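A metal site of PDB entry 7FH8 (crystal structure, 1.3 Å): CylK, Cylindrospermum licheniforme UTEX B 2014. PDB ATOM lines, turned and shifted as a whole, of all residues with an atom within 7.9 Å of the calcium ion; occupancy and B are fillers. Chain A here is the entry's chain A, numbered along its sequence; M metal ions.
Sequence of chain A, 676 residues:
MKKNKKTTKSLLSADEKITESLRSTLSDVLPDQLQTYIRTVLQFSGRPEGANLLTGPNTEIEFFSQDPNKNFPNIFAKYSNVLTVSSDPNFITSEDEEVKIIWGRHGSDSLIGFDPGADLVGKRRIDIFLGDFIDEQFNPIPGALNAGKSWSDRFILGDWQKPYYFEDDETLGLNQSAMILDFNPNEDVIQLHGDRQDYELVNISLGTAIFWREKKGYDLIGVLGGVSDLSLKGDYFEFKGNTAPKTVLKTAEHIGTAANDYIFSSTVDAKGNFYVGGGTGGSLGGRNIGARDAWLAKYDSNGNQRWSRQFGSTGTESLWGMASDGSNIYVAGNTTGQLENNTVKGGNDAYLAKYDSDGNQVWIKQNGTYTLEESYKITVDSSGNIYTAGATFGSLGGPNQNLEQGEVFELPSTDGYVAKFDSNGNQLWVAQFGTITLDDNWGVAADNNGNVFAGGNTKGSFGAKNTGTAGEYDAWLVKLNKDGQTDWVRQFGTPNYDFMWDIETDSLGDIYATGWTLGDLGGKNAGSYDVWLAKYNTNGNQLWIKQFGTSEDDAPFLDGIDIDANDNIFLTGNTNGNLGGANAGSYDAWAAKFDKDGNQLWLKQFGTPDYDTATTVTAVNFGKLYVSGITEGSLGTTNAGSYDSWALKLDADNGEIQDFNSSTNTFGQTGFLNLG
The side-chain hydroxyl (OG1) of Thr 608 lies within hydrogen-bond range of the backbone NH (N) of Asp 610 (2.9 Å). N of Gly 585 sits at hydrogen-bond distance from OD1 of Asn 583, at 2.7 Å. The side-chain carboxylate (OD2) of Asp 588 sits at hydrogen-bond distance from the side-chain amide nitrogen (NE2) of Gln 605, 3.0 Å away. OD1 of Asp 612 sits at hydrogen-bond distance from OG1 of Thr 631 (2.7 Å). The backbone NH (N) of Ala 584 is in hydrogen-bond range of the side-chain carboxylate (OD2) of Asp 588 (2.8 Å). ND2 of Asn 576 lies within hydrogen-bond range of OH of Tyr 587 (3.4 Å). The backbone NH (N) of Asp 588 sits at hydrogen-bond distance from the backbone carbonyl oxygen (O) of Thr 575 (2.8 Å).
Of the 22 residues printed, 6 come within 4 Å of the calcium ion. The nearest printed residue that does not touch the calcium ion is Pro 609 (4.1 Å).
The calcium ion is bound by the side-chain carboxylate (OD1) of Asp 588, 2.3 Å away. The calcium ion is bound by O of Thr 608 (2.3 Å). O of Asp 610 is bound to the calcium ion (2.3 Å). OD2 of Asp 612 binds the calcium ion (2.3 Å). O of Gly 585 is bound to the calcium ion (2.3 Å). The backbone carbonyl oxygen (O) of Tyr 587 is bound to the calcium ion, 2.3 Å away. The calcium ion has six donor atoms within binding distance.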
ATOM      1  N   THR A 575      20.450  -7.313 -25.830  1.00  0.00           N
ATOM      2  CA  THR A 575      21.155  -7.513 -24.575  1.00  0.00           C
ATOM      3  C   THR A 575      20.176  -8.037 -23.537  1.00  0.00           C
ATOM      4  O   THR A 575      19.016  -7.621 -23.519  1.00  0.00           O
ATOM      5  CB  THR A 575      21.791  -6.198 -24.074  1.00  0.00           C
ATOM      6  OG1 THR A 575      22.435  -6.423 -22.815  1.00  0.00           O
ATOM      7  CG2 THR A 575      20.754  -5.105 -23.885  1.00  0.00           C
ATOM      8  N   ASN A 576      20.641  -8.917 -22.662  1.00  0.00           N
ATOM      9  CA  ASN A 576      19.844  -9.252 -21.480  1.00  0.00           C
ATOM     10  C   ASN A 576      20.423  -8.629 -20.219  1.00  0.00           C
ATOM     11  O   ASN A 576      20.071  -9.034 -19.112  1.00  0.00           O
ATOM     12  CB  ASN A 576      19.567 -10.746 -21.360  1.00  0.00           C
ATOM     13  CG  ASN A 576      20.801 -11.559 -21.046  1.00  0.00           C
ATOM     14  OD1 ASN A 576      21.904 -11.003 -20.906  1.00  0.00           O
ATOM     15  ND2 ASN A 576      20.638 -12.874 -20.941  1.00  0.00           N
ATOM     16  N   ASN A 583      17.154  -3.010 -17.707  1.00  0.00           N
ATOM     17  CA  ASN A 583      16.550  -3.992 -18.605  1.00  0.00           C
ATOM     18  C   ASN A 583      15.064  -4.165 -18.290  1.00  0.00           C
ATOM     19  O   ASN A 583      14.671  -4.286 -17.126  1.00  0.00           O
ATOM     20  CB  ASN A 583      17.314  -5.319 -18.470  1.00  0.00           C
ATOM     21  CG  ASN A 583      16.834  -6.358 -19.451  1.00  0.00           C
ATOM     22  OD1 ASN A 583      15.761  -6.922 -19.290  1.00  0.00           O
ATOM     23  ND2 ASN A 583      17.651  -6.632 -20.479  1.00  0.00           N
ATOM     24  N   ALA A 584      14.236  -4.138 -19.338  1.00  0.00           N
ATOM     25  CA  ALA A 584      12.784  -4.220 -19.172  1.00  0.00           C
ATOM     26  C   ALA A 584      12.290  -5.641 -18.938  1.00  0.00           C
ATOM     27  O   ALA A 584      11.176  -5.822 -18.441  1.00  0.00           O
ATOM     28  CB  ALA A 584      12.083  -3.613 -20.396  1.00  0.00           C
ATOM     29  N   GLY A 585      13.097  -6.638 -19.312  1.00  0.00           N
ATOM     30  CA  GLY A 585      12.755  -8.040 -19.142  1.00  0.00           C
ATOM     31  C   GLY A 585      13.289  -8.840 -20.314  1.00  0.00           C
ATOM     32  O   GLY A 585      13.253  -8.376 -21.454  1.00  0.00           O
ATOM     33  N   SER A 586      13.816 -10.026 -20.031  1.00  0.00           N
ATOM     34  CA  SER A 586      14.358 -10.896 -21.090  1.00  0.00           C
ATOM     35  C   SER A 586      15.468 -10.140 -21.849  1.00  0.00           C
ATOM     36  O   SER A 586      16.227  -9.378 -21.238  1.00  0.00           O
ATOM     37  CB  SER A 586      13.200 -11.425 -21.938  1.00  0.00           C
ATOM     38  OG  SER A 586      13.663 -12.289 -22.966  1.00  0.00           O
ATOM     39  N   TYR A 587      15.575 -10.361 -23.159  1.00  0.00           N
ATOM     40  CA  TYR A 587      16.432  -9.514 -23.983  1.00  0.00           C
ATOM     41  C   TYR A 587      15.676  -8.256 -24.380  1.00  0.00           C
ATOM     42  O   TYR A 587      14.439  -8.263 -24.540  1.00  0.00           O
ATOM     43  CB  TYR A 587      16.881 -10.283 -25.243  1.00  0.00           C
ATOM     44  CG  TYR A 587      17.906 -11.355 -24.953  1.00  0.00           C
ATOM     45  CD1 TYR A 587      17.519 -12.578 -24.414  1.00  0.00           C
ATOM     46  CD2 TYR A 587      19.264 -11.147 -25.189  1.00  0.00           C
ATOM     47  CE1 TYR A 587      18.449 -13.555 -24.113  1.00  0.00           C
ATOM     48  CE2 TYR A 587      20.206 -12.116 -24.896  1.00  0.00           C
ATOM     49  CZ  TYR A 587      19.793 -13.329 -24.352  1.00  0.00           C
ATOM     50  OH  TYR A 587      20.696 -14.331 -24.053  1.00  0.00           O
ATOM     51  N   ASP A 588      16.419  -7.166 -24.494  1.00  0.00           N
ATOM     52  CA  ASP A 588      15.923  -5.900 -25.028  1.00  0.00           C
ATOM     53  C   ASP A 588      16.759  -5.534 -26.250  1.00  0.00           C
ATOM     54  O   ASP A 588      17.863  -6.049 -26.457  1.00  0.00           O
ATOM     55  CB  ASP A 588      16.133  -4.753 -24.020  1.00  0.00           C
ATOM     56  CG  ASP A 588      15.194  -4.803 -22.830  1.00  0.00           C
ATOM     57  OD1 ASP A 588      14.180  -5.538 -22.822  1.00  0.00           O
ATOM     58  OD2 ASP A 588      15.502  -4.050 -21.868  1.00  0.00           O
ATOM     59  N   ALA A 589      16.244  -4.615 -27.047  1.00  0.00           N
ATOM     60  CA  ALA A 589      17.032  -4.025 -28.121  1.00  0.00           C
ATOM     61  C   ALA A 589      17.960  -2.934 -27.568  1.00  0.00           C
ATOM     62  O   ALA A 589      17.703  -2.330 -26.527  1.00  0.00           O
ATOM     63  CB  ALA A 589      16.104  -3.377 -29.153  1.00  0.00           C
ATOM     64  N   GLN A 605      18.839   1.837 -24.908  1.00  0.00           N
ATOM     65  CA  GLN A 605      18.226   0.522 -24.809  1.00  0.00           C
ATOM     66  C   GLN A 605      16.726   0.697 -24.720  1.00  0.00           C
ATOM     67  O   GLN A 605      16.249   1.675 -24.132  1.00  0.00           O
ATOM     68  CB  GLN A 605      18.757  -0.224 -23.566  1.00  0.00           C
ATOM     69  CG  GLN A 605      18.229  -1.639 -23.363  1.00  0.00           C
ATOM     70  CD  GLN A 605      19.018  -2.395 -22.297  1.00  0.00           C
ATOM     71  OE1 GLN A 605      20.205  -2.143 -22.116  1.00  0.00           O
ATOM     72  NE2 GLN A 605      18.360  -3.321 -21.595  1.00  0.00           N
ATOM     73  N   PHE A 606      15.973  -0.225 -25.325  1.00  0.00           N
ATOM     74  CA  PHE A 606      14.526  -0.111 -25.363  1.00  0.00           C
ATOM     75  C   PHE A 606      13.911  -1.477 -25.657  1.00  0.00           C
ATOM     76  O   PHE A 606      14.570  -2.366 -26.204  1.00  0.00           O
ATOM     77  CB  PHE A 606      14.068   0.932 -26.392  1.00  0.00           C
ATOM     78  CG  PHE A 606      14.950   0.995 -27.615  1.00  0.00           C
ATOM     79  CD1 PHE A 606      14.809   0.075 -28.643  1.00  0.00           C
ATOM     80  CD2 PHE A 606      15.967   1.941 -27.716  1.00  0.00           C
ATOM     81  CE1 PHE A 606      15.632   0.125 -29.759  1.00  0.00           C
ATOM     82  CE2 PHE A 606      16.800   1.983 -28.825  1.00  0.00           C
ATOM     83  CZ  PHE A 606      16.632   1.075 -29.847  1.00  0.00           C
ATOM     84  N   GLY A 607      12.647  -1.625 -25.304  1.00  0.00           N
ATOM     85  CA  GLY A 607      11.961  -2.876 -25.547  1.00  0.00           C
ATOM     86  C   GLY A 607      10.804  -3.085 -24.601  1.00  0.00           C
ATOM     87  O   GLY A 607      10.258  -2.128 -24.049  1.00  0.00           O
ATOM     88  N   THR A 608      10.405  -4.343 -24.467  1.00  0.00           N
ATOM     89  CA  THR A 608       9.248  -4.732 -23.685  1.00  0.00           C
ATOM     90  C   THR A 608       9.714  -5.655 -22.557  1.00  0.00           C
ATOM     91  O   THR A 608      10.873  -6.077 -22.538  1.00  0.00           O
ATOM     92  CB  THR A 608       8.238  -5.508 -24.553  1.00  0.00           C
ATOM     93  OG1 THR A 608       8.698  -6.858 -24.758  1.00  0.00           O
ATOM     94  CG2 THR A 608       7.960  -4.826 -25.896  1.00  0.00           C
ATOM     95  N   PRO A 609       8.822  -6.019 -21.622  1.00  0.00           N
ATOM     96  CA  PRO A 609       9.178  -7.042 -20.627  1.00  0.00           C
ATOM     97  C   PRO A 609       9.432  -8.417 -21.226  1.00  0.00           C
ATOM     98  O   PRO A 609       9.951  -9.292 -20.528  1.00  0.00           O
ATOM     99  CB  PRO A 609       7.950  -7.088 -19.719  1.00  0.00           C
ATOM    100  CG  PRO A 609       7.380  -5.672 -19.817  1.00  0.00           C
ATOM    101  CD  PRO A 609       7.543  -5.365 -21.284  1.00  0.00           C
ATOM    102  N   ASP A 610       9.080  -8.637 -22.488  1.00  0.00           N
ATOM    103  CA  ASP A 610       9.278  -9.915 -23.153  1.00  0.00           C
ATOM    104  C   ASP A 610      10.525  -9.855 -24.033  1.00  0.00           C
ATOM    105  O   ASP A 610      11.263  -8.861 -24.041  1.00  0.00           O
ATOM    106  CB  ASP A 610       8.004 -10.269 -23.902  1.00  0.00           C
ATOM    107  CG  ASP A 610       6.841 -10.465 -22.976  1.00  0.00           C
ATOM    108  OD1 ASP A 610       6.994 -11.185 -21.972  1.00  0.00           O
ATOM    109  OD2 ASP A 610       5.798  -9.830 -23.210  1.00  0.00           O
ATOM    110  N   TYR A 611      10.753 -10.923 -24.801  1.00  0.00           N
ATOM    111  CA  TYR A 611      11.925 -11.010 -25.673  1.00  0.00           C
ATOM    112  C   TYR A 611      11.837  -9.976 -26.802  1.00  0.00           C
ATOM    113  O   TYR A 611      10.846  -9.950 -27.539  1.00  0.00           O
ATOM    114  CB  TYR A 611      12.045 -12.411 -26.280  1.00  0.00           C
ATOM    115  CG  TYR A 611      13.275 -12.505 -27.156  1.00  0.00           C
ATOM    116  CD1 TYR A 611      14.510 -12.855 -26.610  1.00  0.00           C
ATOM    117  CD2 TYR A 611      13.207 -12.211 -28.528  1.00  0.00           C
ATOM    118  CE1 TYR A 611      15.646 -12.902 -27.384  1.00  0.00           C
ATOM    119  CE2 TYR A 611      14.349 -12.237 -29.307  1.00  0.00           C
ATOM    120  CZ  TYR A 611      15.565 -12.589 -28.735  1.00  0.00           C
ATOM    121  OH  TYR A 611      16.699 -12.627 -29.514  1.00  0.00           O
ATOM    122  N   ASP A 612      12.874  -9.150 -26.929  1.00  0.00           N
ATOM    123  CA  ASP A 612      13.010  -8.269 -28.079  1.00  0.00           C
ATOM    124  C   ASP A 612      14.448  -8.321 -28.576  1.00  0.00           C
ATOM    125  O   ASP A 612      15.380  -8.504 -27.782  1.00  0.00           O
ATOM    126  CB  ASP A 612      12.728  -6.788 -27.734  1.00  0.00           C
ATOM    127  CG  ASP A 612      11.769  -6.625 -26.578  1.00  0.00           C
ATOM    128  OD1 ASP A 612      10.557  -6.851 -26.770  1.00  0.00           O
ATOM    129  OD2 ASP A 612      12.239  -6.235 -25.478  1.00  0.00           O
ATOM    130  N   THR A 613      14.624  -8.130 -29.884  1.00  0.00           N
ATOM    131  CA  THR A 613      15.941  -7.810 -30.432  1.00  0.00           C
ATOM    132  C   THR A 613      15.780  -6.865 -31.597  1.00  0.00           C
ATOM    133  O   THR A 613      14.849  -6.997 -32.384  1.00  0.00           O
ATOM    134  CB  THR A 613      16.750  -9.055 -30.873  1.00  0.00           C
ATOM    135  OG1 THR A 613      18.039  -8.625 -31.336  1.00  0.00           O
ATOM    136  CG2 THR A 613      16.044  -9.859 -31.995  1.00  0.00           C
ATOM    137  N   THR A 631       9.829  -8.887 -31.779  1.00  0.00           N
ATOM    138  CA  THR A 631       9.446  -8.979 -30.374  1.00  0.00           C
ATOM    139  C   THR A 631       8.391 -10.068 -30.164  1.00  0.00           C
ATOM    140  O   THR A 631       7.547 -10.327 -31.037  1.00  0.00           O
ATOM    141  CB  THR A 631       8.919  -7.628 -29.849  1.00  0.00           C
ATOM    142  OG1 THR A 631       8.681  -7.727 -28.442  1.00  0.00           O
ATOM    143  CG2 THR A 631       7.608  -7.221 -30.525  1.00  0.00           C
ATOM    144  N   GLU A 632       8.425 -10.658 -28.963  1.00  0.00           N
ATOM    145  CA  GLU A 632       7.333 -11.482 -28.464  1.00  0.00           C
ATOM    146  C   GLU A 632       6.382 -10.665 -27.594  1.00  0.00           C
ATOM    147  O   GLU A 632       5.357 -11.191 -27.154  1.00  0.00           O
ATOM    148  CB  GLU A 632       7.883 -12.634 -27.630  1.00  0.00           C
ATOM    149  CG  GLU A 632       8.768 -13.609 -28.422  1.00  0.00           C
ATOM    150  CD  GLU A 632       9.444 -14.631 -27.543  1.00  0.00           C
ATOM    151  OE1 GLU A 632       8.888 -14.969 -26.467  1.00  0.00           O
ATOM    152  OE2 GLU A 632      10.557 -15.089 -27.897  1.00  0.00           O
ATOM    153  N   GLY A 633       6.690  -9.395 -27.329  1.00  0.00           N
ATOM    154  CA  GLY A 633       5.829  -8.533 -26.551  1.00  0.00           C
ATOM    155  C   GLY A 633       4.914  -7.705 -27.423  1.00  0.00           C
ATOM    156  O   GLY A 633       4.735  -7.959 -28.624  1.00  0.00           O
ATOM    157  N   LEU A 635       4.765  -4.230 -28.711  1.00  0.00           N
ATOM    158  CA  LEU A 635       5.614  -3.062 -28.922  1.00  0.00           C
ATOM    159  C   LEU A 635       4.966  -2.262 -30.042  1.00  0.00           C
ATOM    160  O   LEU A 635       4.942  -2.721 -31.194  1.00  0.00           O
ATOM    161  CB  LEU A 635       7.045  -3.477 -29.245  1.00  0.00           C
ATOM    162  CG  LEU A 635       8.136  -2.437 -28.970  1.00  0.00           C
ATOM    163  CD1 LEU A 635       9.519  -3.066 -29.021  1.00  0.00           C
ATOM    164  CD2 LEU A 635       8.065  -1.269 -29.944  1.00  0.00           C
HETATM  165 CA    CA M   1      12.705  -7.177 -23.389  1.00  0.00          CA
